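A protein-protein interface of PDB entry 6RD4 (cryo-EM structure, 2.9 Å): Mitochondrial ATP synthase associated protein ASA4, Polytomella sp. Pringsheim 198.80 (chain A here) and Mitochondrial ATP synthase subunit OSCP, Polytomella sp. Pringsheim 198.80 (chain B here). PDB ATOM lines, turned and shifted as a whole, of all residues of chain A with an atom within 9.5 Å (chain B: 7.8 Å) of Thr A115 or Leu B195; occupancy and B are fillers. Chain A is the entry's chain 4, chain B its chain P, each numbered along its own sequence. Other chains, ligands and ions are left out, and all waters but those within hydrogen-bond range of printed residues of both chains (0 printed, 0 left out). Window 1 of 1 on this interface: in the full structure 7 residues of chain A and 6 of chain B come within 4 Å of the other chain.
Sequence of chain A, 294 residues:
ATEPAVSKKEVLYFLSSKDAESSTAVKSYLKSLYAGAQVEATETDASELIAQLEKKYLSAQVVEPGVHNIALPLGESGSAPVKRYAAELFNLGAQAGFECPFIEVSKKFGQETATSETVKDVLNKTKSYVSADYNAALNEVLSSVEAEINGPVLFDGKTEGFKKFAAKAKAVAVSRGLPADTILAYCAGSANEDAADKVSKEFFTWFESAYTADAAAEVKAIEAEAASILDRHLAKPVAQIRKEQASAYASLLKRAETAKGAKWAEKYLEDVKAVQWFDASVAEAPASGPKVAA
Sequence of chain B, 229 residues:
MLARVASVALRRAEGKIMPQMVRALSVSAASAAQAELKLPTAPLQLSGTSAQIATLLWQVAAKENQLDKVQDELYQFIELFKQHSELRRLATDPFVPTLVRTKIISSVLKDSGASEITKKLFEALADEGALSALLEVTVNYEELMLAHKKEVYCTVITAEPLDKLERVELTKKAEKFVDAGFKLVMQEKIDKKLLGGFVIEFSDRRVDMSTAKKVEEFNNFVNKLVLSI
The side-chain amino group (NZ) of Lys B193 lies within salt-bridge range of the side-chain carboxylate (OE1) of Glu A117.
The side-chain amino group of Lys B193 lies within hydrogen-bond range of the backbone carbonyl oxygen of Thr A115 (2.8 Å).
The side-chain carboxylate of Asp A121 is in hydrogen-bond range of the side-chain hydroxyl of Ser A116 (2.9 Å).
The backbone NH (N) of Phe A155 is in hydrogen-bond range of the backbone carbonyl oxygen (O) of Glu A117, 2.4 Å away.
Among the printed residues, merely in contact across the chains: Thr A115 with Lys B192 (3.9 Å), Thr A115 with Leu B195 (3.7 Å) and Ser A116 with Lys B193 (3.8 Å).
Of chain B, only Lys B192 (3.9 Å), Lys B193 (2.8 Å) and Leu B195 (3.7 Å) come within 4 Å of Thr A115.
Printed residues of chain A within 4 Å of Leu B195: Thr A115.
No residue of chain B comes within 4 Å of Ala A114.
No residue of chain A comes within 4 Å of Gly B196.
No residue of chain A comes within 4 Å of Thr B211.
Printed residues of chain B within 4 Å of Glu A117: Lys B193 (3.6 Å).
Printed residues of chain B within 4 Å of Ser A116: Lys B193.
Of the printed residues of chain A, Lys B192 touches Thr A115 (3.9 Å).
Asp B191 touches none of the printed residues of chain A.
The nearest residue of chain B that does not touch Thr A115 is Leu B194 (5.3 Å).
The nearest residue of chain A that does not touch Leu B195 is Ala A114 (4.6 Å).
Of the 17 printed residues of chain B, 3 touch a printed residue of chain A.
Printed residues of chain B that touch a printed residue of chain A: Lys B192, Lys B193 and Leu B195.
Hydrophobic or aromatic side chains of chain B within 4 Å of the printed part of chain A: Leu B195.
Of the 16 printed residues of chain A, 3 touch a printed residue of chain B.
Among the printed residues, 5 pairs touch across the chains.
Among the printed residues, Asp or Glu carboxylates within 4 Å of a Lys or Arg side-chain nitrogen of the other chain: Glu A117 with Lys B193.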
ATOM      1  N   LEU A  49     -27.027   4.693  40.809  1.00  0.00           N
ATOM      2  CA  LEU A  49     -26.139   5.512  39.995  1.00  0.00           C
ATOM      3  C   LEU A  49     -25.637   6.732  40.753  1.00  0.00           C
ATOM      4  O   LEU A  49     -24.512   7.177  40.521  1.00  0.00           O
ATOM      5  CB  LEU A  49     -26.846   5.948  38.718  1.00  0.00           C
ATOM      6  CG  LEU A  49     -27.068   4.879  37.654  1.00  0.00           C
ATOM      7  CD1 LEU A  49     -27.827   5.470  36.485  1.00  0.00           C
ATOM      8  CD2 LEU A  49     -25.745   4.304  37.200  1.00  0.00           C
ATOM      9  N   PHE A 109     -14.090  -5.138  35.020  1.00  0.00           N
ATOM     10  CA  PHE A 109     -14.287  -5.948  33.828  1.00  0.00           C
ATOM     11  C   PHE A 109     -15.728  -6.417  33.725  1.00  0.00           C
ATOM     12  O   PHE A 109     -16.408  -6.148  32.731  1.00  0.00           O
ATOM     13  CB  PHE A 109     -13.351  -7.146  33.849  1.00  0.00           C
ATOM     14  CG  PHE A 109     -11.921  -6.801  33.676  1.00  0.00           C
ATOM     15  CD1 PHE A 109     -11.545  -5.720  32.925  1.00  0.00           C
ATOM     16  CD2 PHE A 109     -10.946  -7.576  34.251  1.00  0.00           C
ATOM     17  CE1 PHE A 109     -10.226  -5.419  32.760  1.00  0.00           C
ATOM     18  CE2 PHE A 109      -9.630  -7.270  34.088  1.00  0.00           C
ATOM     19  CZ  PHE A 109      -9.272  -6.190  33.341  1.00  0.00           C
ATOM     20  N   GLY A 110     -16.225  -7.078  34.769  1.00  0.00           N
ATOM     21  CA  GLY A 110     -17.560  -7.638  34.745  1.00  0.00           C
ATOM     22  C   GLY A 110     -18.668  -6.614  34.754  1.00  0.00           C
ATOM     23  O   GLY A 110     -19.814  -6.960  34.465  1.00  0.00           O
ATOM     24  N   GLN A 111     -18.365  -5.368  35.093  1.00  0.00           N
ATOM     25  CA  GLN A 111     -19.355  -4.312  34.963  1.00  0.00           C
ATOM     26  C   GLN A 111     -19.390  -3.770  33.543  1.00  0.00           C
ATOM     27  O   GLN A 111     -20.466  -3.483  33.013  1.00  0.00           O
ATOM     28  CB  GLN A 111     -19.057  -3.202  35.965  1.00  0.00           C
ATOM     29  CG  GLN A 111     -19.724  -1.881  35.711  1.00  0.00           C
ATOM     30  CD  GLN A 111     -19.072  -0.770  36.494  1.00  0.00           C
ATOM     31  OE1 GLN A 111     -18.665  -0.963  37.638  1.00  0.00           O
ATOM     32  NE2 GLN A 111     -18.950   0.396  35.878  1.00  0.00           N
ATOM     33  N   GLU A 112     -18.229  -3.643  32.904  1.00  0.00           N
ATOM     34  CA  GLU A 112     -18.198  -3.107  31.550  1.00  0.00           C
ATOM     35  C   GLU A 112     -18.696  -4.119  30.529  1.00  0.00           C
ATOM     36  O   GLU A 112     -19.180  -3.730  29.464  1.00  0.00           O
ATOM     37  CB  GLU A 112     -16.785  -2.651  31.189  1.00  0.00           C
ATOM     38  CG  GLU A 112     -16.358  -1.354  31.846  1.00  0.00           C
ATOM     39  CD  GLU A 112     -17.092  -0.152  31.302  1.00  0.00           C
ATOM     40  OE1 GLU A 112     -17.488  -0.177  30.119  1.00  0.00           O
ATOM     41  OE2 GLU A 112     -17.271   0.826  32.057  1.00  0.00           O
ATOM     42  N   THR A 113     -18.599  -5.409  30.835  1.00  0.00           N
ATOM     43  CA  THR A 113     -19.016  -6.447  29.905  1.00  0.00           C
ATOM     44  C   THR A 113     -20.165  -7.275  30.456  1.00  0.00           C
ATOM     45  O   THR A 113     -20.132  -8.507  30.382  1.00  0.00           O
ATOM     46  CB  THR A 113     -17.853  -7.368  29.574  1.00  0.00           C
ATOM     47  OG1 THR A 113     -17.287  -7.853  30.788  1.00  0.00           O
ATOM     48  CG2 THR A 113     -16.801  -6.626  28.817  1.00  0.00           C
ATOM     49  N   ALA A 114     -21.175  -6.632  31.031  1.00  0.00           N
ATOM     50  CA  ALA A 114     -22.340  -7.377  31.487  1.00  0.00           C
ATOM     51  C   ALA A 114     -23.325  -7.666  30.363  1.00  0.00           C
ATOM     52  O   ALA A 114     -24.264  -8.443  30.566  1.00  0.00           O
ATOM     53  CB  ALA A 114     -23.049  -6.618  32.606  1.00  0.00           C
ATOM     54  N   THR A 115     -23.131  -7.067  29.193  1.00  0.00           N
ATOM     55  CA  THR A 115     -24.045  -7.196  28.069  1.00  0.00           C
ATOM     56  C   THR A 115     -23.504  -8.111  26.987  1.00  0.00           C
ATOM     57  O   THR A 115     -24.207  -8.388  26.013  1.00  0.00           O
ATOM     58  CB  THR A 115     -24.326  -5.823  27.464  1.00  0.00           C
ATOM     59  OG1 THR A 115     -23.085  -5.208  27.095  1.00  0.00           O
ATOM     60  CG2 THR A 115     -25.019  -4.939  28.469  1.00  0.00           C
ATOM     61  N   SER A 116     -22.276  -8.583  27.126  1.00  0.00           N
ATOM     62  CA  SER A 116     -21.550  -9.198  26.030  1.00  0.00           C
ATOM     63  C   SER A 116     -21.625 -10.710  26.139  1.00  0.00           C
ATOM     64  O   SER A 116     -21.464 -11.268  27.228  1.00  0.00           O
ATOM     65  CB  SER A 116     -20.094  -8.740  26.031  1.00  0.00           C
ATOM     66  OG  SER A 116     -20.009  -7.333  26.168  1.00  0.00           O
ATOM     67  N   GLU A 117     -21.881 -11.365  25.009  1.00  0.00           N
ATOM     68  CA  GLU A 117     -21.804 -12.816  24.937  1.00  0.00           C
ATOM     69  C   GLU A 117     -20.829 -13.281  23.867  1.00  0.00           C
ATOM     70  O   GLU A 117     -20.656 -14.493  23.692  1.00  0.00           O
ATOM     71  CB  GLU A 117     -23.188 -13.431  24.696  1.00  0.00           C
ATOM     72  CG  GLU A 117     -23.894 -12.931  23.450  1.00  0.00           C
ATOM     73  CD  GLU A 117     -24.841 -11.779  23.750  1.00  0.00           C
ATOM     74  OE1 GLU A 117     -24.797 -11.245  24.876  1.00  0.00           O
ATOM     75  OE2 GLU A 117     -25.625 -11.400  22.858  1.00  0.00           O
ATOM     76  N   THR A 118     -20.177 -12.367  23.163  1.00  0.00           N
ATOM     77  CA  THR A 118     -19.104 -12.698  22.245  1.00  0.00           C
ATOM     78  C   THR A 118     -17.784 -12.151  22.764  1.00  0.00           C
ATOM     79  O   THR A 118     -17.740 -11.124  23.443  1.00  0.00           O
ATOM     80  CB  THR A 118     -19.383 -12.151  20.851  1.00  0.00           C
ATOM     81  OG1 THR A 118     -18.198 -12.260  20.059  1.00  0.00           O
ATOM     82  CG2 THR A 118     -19.837 -10.709  20.922  1.00  0.00           C
ATOM     83  N   VAL A 119     -16.705 -12.850  22.426  1.00  0.00           N
ATOM     84  CA  VAL A 119     -15.393 -12.516  22.965  1.00  0.00           C
ATOM     85  C   VAL A 119     -14.828 -11.271  22.295  1.00  0.00           C
ATOM     86  O   VAL A 119     -14.160 -10.465  22.946  1.00  0.00           O
ATOM     87  CB  VAL A 119     -14.481 -13.744  22.825  1.00  0.00           C
ATOM     88  CG1 VAL A 119     -13.065 -13.440  23.193  1.00  0.00           C
ATOM     89  CG2 VAL A 119     -14.989 -14.837  23.719  1.00  0.00           C
ATOM     90  N   ASP A 121     -16.384  -8.667  21.521  1.00  0.00           N
ATOM     91  CA  ASP A 121     -16.898  -7.490  22.202  1.00  0.00           C
ATOM     92  C   ASP A 121     -16.359  -7.391  23.621  1.00  0.00           C
ATOM     93  O   ASP A 121     -16.225  -6.285  24.147  1.00  0.00           O
ATOM     94  CB  ASP A 121     -18.425  -7.519  22.172  1.00  0.00           C
ATOM     95  CG  ASP A 121     -19.051  -6.230  22.639  1.00  0.00           C
ATOM     96  OD1 ASP A 121     -19.033  -5.938  23.847  1.00  0.00           O
ATOM     97  OD2 ASP A 121     -19.561  -5.489  21.780  1.00  0.00           O
ATOM     98  N   VAL A 122     -16.033  -8.521  24.248  1.00  0.00           N
ATOM     99  CA  VAL A 122     -15.395  -8.491  25.561  1.00  0.00           C
ATOM    100  C   VAL A 122     -13.994  -7.907  25.455  1.00  0.00           C
ATOM    101  O   VAL A 122     -13.612  -7.023  26.225  1.00  0.00           O
ATOM    102  CB  VAL A 122     -15.378  -9.899  26.174  1.00  0.00           C
ATOM    103  CG1 VAL A 122     -14.403  -9.987  27.317  1.00  0.00           C
ATOM    104  CG2 VAL A 122     -16.751 -10.252  26.645  1.00  0.00           C
ATOM    105  N   LYS A 125     -14.535  -3.645  24.787  1.00  0.00           N
ATOM    106  CA  LYS A 125     -14.904  -2.649  25.783  1.00  0.00           C
ATOM    107  C   LYS A 125     -14.218  -2.883  27.122  1.00  0.00           C
ATOM    108  O   LYS A 125     -14.484  -2.150  28.075  1.00  0.00           O
ATOM    109  CB  LYS A 125     -16.418  -2.580  25.965  1.00  0.00           C
ATOM    110  CG  LYS A 125     -17.105  -3.899  26.168  1.00  0.00           C
ATOM    111  CD  LYS A 125     -18.611  -3.732  26.249  1.00  0.00           C
ATOM    112  CE  LYS A 125     -19.158  -2.866  25.129  1.00  0.00           C
ATOM    113  NZ  LYS A 125     -20.644  -2.893  25.072  1.00  0.00           N
ATOM    114  N   PHE A 155     -18.768 -15.863  24.432  1.00  0.00           N
ATOM    115  CA  PHE A 155     -18.430 -15.736  25.845  1.00  0.00           C
ATOM    116  C   PHE A 155     -19.398 -16.620  26.634  1.00  0.00           C
ATOM    117  O   PHE A 155     -20.335 -16.160  27.286  1.00  0.00           O
ATOM    118  CB  PHE A 155     -18.501 -14.272  26.260  1.00  0.00           C
ATOM    119  CG  PHE A 155     -17.650 -13.926  27.438  1.00  0.00           C
ATOM    120  CD1 PHE A 155     -16.369 -14.428  27.557  1.00  0.00           C
ATOM    121  CD2 PHE A 155     -18.121 -13.057  28.408  1.00  0.00           C
ATOM    122  CE1 PHE A 155     -15.586 -14.098  28.634  1.00  0.00           C
ATOM    123  CE2 PHE A 155     -17.337 -12.712  29.478  1.00  0.00           C
ATOM    124  CZ  PHE A 155     -16.074 -13.246  29.597  1.00  0.00           C
ATOM    125  N   THR B 158     -37.563  -6.322  26.298  1.00  0.00           N
ATOM    126  CA  THR B 158     -37.128  -6.316  27.685  1.00  0.00           C
ATOM    127  C   THR B 158     -35.822  -7.093  27.815  1.00  0.00           C
ATOM    128  O   THR B 158     -35.225  -7.515  26.830  1.00  0.00           O
ATOM    129  CB  THR B 158     -38.215  -6.899  28.588  1.00  0.00           C
ATOM    130  OG1 THR B 158     -38.622  -8.169  28.069  1.00  0.00           O
ATOM    131  CG2 THR B 158     -39.407  -5.981  28.650  1.00  0.00           C
ATOM    132  N   ALA B 159     -35.366  -7.267  29.053  1.00  0.00           N
ATOM    133  CA  ALA B 159     -34.081  -7.920  29.271  1.00  0.00           C
ATOM    134  C   ALA B 159     -34.239  -9.434  29.394  1.00  0.00           C
ATOM    135  O   ALA B 159     -33.541 -10.200  28.723  1.00  0.00           O
ATOM    136  CB  ALA B 159     -33.405  -7.330  30.510  1.00  0.00           C
ATOM    137  N   GLU B 160     -35.138  -9.877  30.259  1.00  0.00           N
ATOM    138  CA  GLU B 160     -35.534 -11.268  30.393  1.00  0.00           C
ATOM    139  C   GLU B 160     -37.050 -11.318  30.281  1.00  0.00           C
ATOM    140  O   GLU B 160     -37.707 -10.279  30.401  1.00  0.00           O
ATOM    141  CB  GLU B 160     -35.047 -11.850  31.733  1.00  0.00           C
ATOM    142  CG  GLU B 160     -35.732 -11.300  32.963  1.00  0.00           C
ATOM    143  CD  GLU B 160     -35.012 -10.107  33.553  1.00  0.00           C
ATOM    144  OE1 GLU B 160     -34.151  -9.525  32.867  1.00  0.00           O
ATOM    145  OE2 GLU B 160     -35.300  -9.754  34.713  1.00  0.00           O
ATOM    146  N   ASP B 191     -33.853  -8.810  25.088  1.00  0.00           N
ATOM    147  CA  ASP B 191     -32.494  -8.378  24.749  1.00  0.00           C
ATOM    148  C   ASP B 191     -31.759  -8.054  26.048  1.00  0.00           C
ATOM    149  O   ASP B 191     -32.083  -7.067  26.708  1.00  0.00           O
ATOM    150  CB  ASP B 191     -32.506  -7.175  23.824  1.00  0.00           C
ATOM    151  CG  ASP B 191     -31.284  -7.117  22.934  1.00  0.00           C
ATOM    152  OD1 ASP B 191     -31.211  -6.204  22.089  1.00  0.00           O
ATOM    153  OD2 ASP B 191     -30.390  -7.978  23.085  1.00  0.00           O
ATOM    154  N   LYS B 192     -30.766  -8.871  26.391  1.00  0.00           N
ATOM    155  CA  LYS B 192     -29.954  -8.584  27.566  1.00  0.00           C
ATOM    156  C   LYS B 192     -28.856  -7.560  27.308  1.00  0.00           C
ATOM    157  O   LYS B 192     -28.086  -7.260  28.224  1.00  0.00           O
ATOM    158  CB  LYS B 192     -29.360  -9.873  28.122  1.00  0.00           C
ATOM    159  CG  LYS B 192     -28.569 -10.691  27.132  1.00  0.00           C
ATOM    160  CD  LYS B 192     -27.965 -11.893  27.831  1.00  0.00           C
ATOM    161  CE  LYS B 192     -29.045 -12.807  28.393  1.00  0.00           C
ATOM    162  NZ  LYS B 192     -29.913 -13.400  27.348  1.00  0.00           N
ATOM    163  N   LYS B 193     -28.773  -7.005  26.097  1.00  0.00           N
ATOM    164  CA  LYS B 193     -28.046  -5.757  25.910  1.00  0.00           C
ATOM    165  C   LYS B 193     -28.727  -4.614  26.652  1.00  0.00           C
ATOM    166  O   LYS B 193     -28.083  -3.613  26.977  1.00  0.00           O
ATOM    167  CB  LYS B 193     -27.929  -5.438  24.423  1.00  0.00           C
ATOM    168  CG  LYS B 193     -27.357  -6.569  23.584  1.00  0.00           C
ATOM    169  CD  LYS B 193     -25.838  -6.599  23.625  1.00  0.00           C
ATOM    170  CE  LYS B 193     -25.301  -7.840  22.924  1.00  0.00           C
ATOM    171  NZ  LYS B 193     -23.859  -8.087  23.206  1.00  0.00           N
ATOM    172  N   LEU B 194     -30.029  -4.726  26.883  1.00  0.00           N
ATOM    173  CA  LEU B 194     -30.711  -3.882  27.848  1.00  0.00           C
ATOM    174  C   LEU B 194     -30.472  -4.431  29.245  1.00  0.00           C
ATOM    175  O   LEU B 194     -30.510  -5.644  29.460  1.00  0.00           O
ATOM    176  CB  LEU B 194     -32.207  -3.849  27.555  1.00  0.00           C
ATOM    177  CG  LEU B 194     -32.857  -2.875  26.577  1.00  0.00           C
ATOM    178  CD1 LEU B 194     -32.307  -2.988  25.169  1.00  0.00           C
ATOM    179  CD2 LEU B 194     -34.341  -3.146  26.575  1.00  0.00           C
ATOM    180  N   LEU B 195     -30.196  -3.546  30.193  1.00  0.00           N
ATOM    181  CA  LEU B 195     -30.069  -3.934  31.597  1.00  0.00           C
ATOM    182  C   LEU B 195     -31.341  -3.602  32.366  1.00  0.00           C
ATOM    183  O   LEU B 195     -31.339  -2.834  33.323  1.00  0.00           O
ATOM    184  CB  LEU B 195     -28.860  -3.258  32.229  1.00  0.00           C
ATOM    185  CG  LEU B 195     -27.566  -3.352  31.448  1.00  0.00           C
ATOM    186  CD1 LEU B 195     -26.509  -2.503  32.101  1.00  0.00           C
ATOM    187  CD2 LEU B 195     -27.161  -4.799  31.452  1.00  0.00           C
ATOM    188  N   GLY B 196     -32.443  -4.190  31.940  1.00  0.00           N
ATOM    189  CA  GLY B 196     -33.702  -3.921  32.593  1.00  0.00           C
ATOM    190  C   GLY B 196     -34.344  -2.640  32.092  1.00  0.00           C
ATOM    191  O   GLY B 196     -33.724  -1.810  31.434  1.00  0.00           O
ATOM    192  N   GLY B 197     -35.613  -2.478  32.442  1.00  0.00           N
ATOM    193  CA  GLY B 197     -36.428  -1.480  31.789  1.00  0.00           C
ATOM    194  C   GLY B 197     -36.984  -2.098  30.527  1.00  0.00           C
ATOM    195  O   GLY B 197     -37.074  -3.325  30.435  1.00  0.00           O
ATOM    196  N   PHE B 198     -37.331  -1.283  29.538  1.00  0.00           N
ATOM    197  CA  PHE B 198     -37.911  -1.813  28.315  1.00  0.00           C
ATOM    198  C   PHE B 198     -37.700  -0.815  27.192  1.00  0.00           C
ATOM    199  O   PHE B 198     -37.340   0.341  27.420  1.00  0.00           O
ATOM    200  CB  PHE B 198     -39.403  -2.111  28.476  1.00  0.00           C
ATOM    201  CG  PHE B 198     -40.149  -1.056  29.226  1.00  0.00           C
ATOM    202  CD1 PHE B 198     -40.375  -1.181  30.579  1.00  0.00           C
ATOM    203  CD2 PHE B 198     -40.644   0.055  28.574  1.00  0.00           C
ATOM    204  CE1 PHE B 198     -41.060  -0.215  31.269  1.00  0.00           C
ATOM    205  CE2 PHE B 198     -41.333   1.021  29.257  1.00  0.00           C
ATOM    206  CZ  PHE B 198     -41.541   0.884  30.607  1.00  0.00           C
ATOM    207  N   MET B 209     -37.296   3.591  27.908  1.00  0.00           N
ATOM    208  CA  MET B 209     -37.121   3.703  29.346  1.00  0.00           C
ATOM    209  C   MET B 209     -36.325   2.547  29.908  1.00  0.00           C
ATOM    210  O   MET B 209     -36.470   2.207  31.088  1.00  0.00           O
ATOM    211  CB  MET B 209     -38.471   3.835  30.049  1.00  0.00           C
ATOM    212  CG  MET B 209     -39.182   5.126  29.711  1.00  0.00           C
ATOM    213  SD  MET B 209     -40.527   5.587  30.816  1.00  0.00           S
ATOM    214  CE  MET B 209     -41.793   4.427  30.345  1.00  0.00           C
ATOM    215  N   SER B 210     -35.489   1.925  29.084  1.00  0.00           N
ATOM    216  CA  SER B 210     -34.574   0.913  29.568  1.00  0.00           C
ATOM    217  C   SER B 210     -33.463   1.561  30.370  1.00  0.00           C
ATOM    218  O   SER B 210     -33.069   2.698  30.112  1.00  0.00           O
ATOM    219  CB  SER B 210     -33.974   0.136  28.405  1.00  0.00           C
ATOM    220  OG  SER B 210     -33.095   0.952  27.660  1.00  0.00           O
ATOM    221  N   THR B 211     -32.946   0.823  31.351  1.00  0.00           N
ATOM    222  CA  THR B 211     -31.883   1.372  32.176  1.00  0.00           C
ATOM    223  C   THR B 211     -30.518   1.253  31.526  1.00  0.00           C
ATOM    224  O   THR B 211     -29.562   1.831  32.038  1.00  0.00           O
ATOM    225  CB  THR B 211     -31.847   0.704  33.552  1.00  0.00           C
ATOM    226  OG1 THR B 211     -31.164  -0.551  33.460  1.00  0.00           O
ATOM    227  CG2 THR B 211     -33.251   0.480  34.076  1.00  0.00           C
ATOM    228  N   ALA B 212     -30.398   0.512  30.427  1.00  0.00           N
ATOM    229  CA  ALA B 212     -29.132   0.488  29.704  1.00  0.00           C
ATOM    230  C   ALA B 212     -28.860   1.820  29.034  1.00  0.00           C
ATOM    231  O   ALA B 212     -27.702   2.221  28.893  1.00  0.00           O
ATOM    232  CB  ALA B 212     -29.120  -0.633  28.675  1.00  0.00           C
ATOM    233  N   LYS B 213     -29.906   2.503  28.576  1.00  0.00           N
ATOM    234  CA  LYS B 213     -29.726   3.862  28.086  1.00  0.00           C
ATOM    235  C   LYS B 213     -29.796   4.886  29.208  1.00  0.00           C
ATOM    236  O   LYS B 213     -29.234   5.975  29.074  1.00  0.00           O
ATOM    237  CB  LYS B 213     -30.768   4.191  27.017  1.00  0.00           C
ATOM    238  CG  LYS B 213     -30.373   5.355  26.121  1.00  0.00           C
ATOM    239  CD  LYS B 213     -31.451   5.694  25.136  1.00  0.00           C
ATOM    240  CE  LYS B 213     -32.557   6.459  25.818  1.00  0.00           C
ATOM    241  NZ  LYS B 213     -32.095   7.792  26.266  1.00  0.00           N
ATOM    242  N   VAL B 215     -28.266   4.541  31.941  1.00  0.00           N
ATOM    243  CA  VAL B 215     -26.856   4.640  32.304  1.00  0.00           C
ATOM    244  C   VAL B 215     -26.150   5.653  31.414  1.00  0.00           C
ATOM    245  O   VAL B 215     -25.500   6.582  31.905  1.00  0.00           O
ATOM    246  CB  VAL B 215     -26.186   3.258  32.219  1.00  0.00           C
ATOM    247  CG1 VAL B 215     -24.695   3.393  32.294  1.00  0.00           C
ATOM    248  CG2 VAL B 215     -26.656   2.393  33.352  1.00  0.00           C
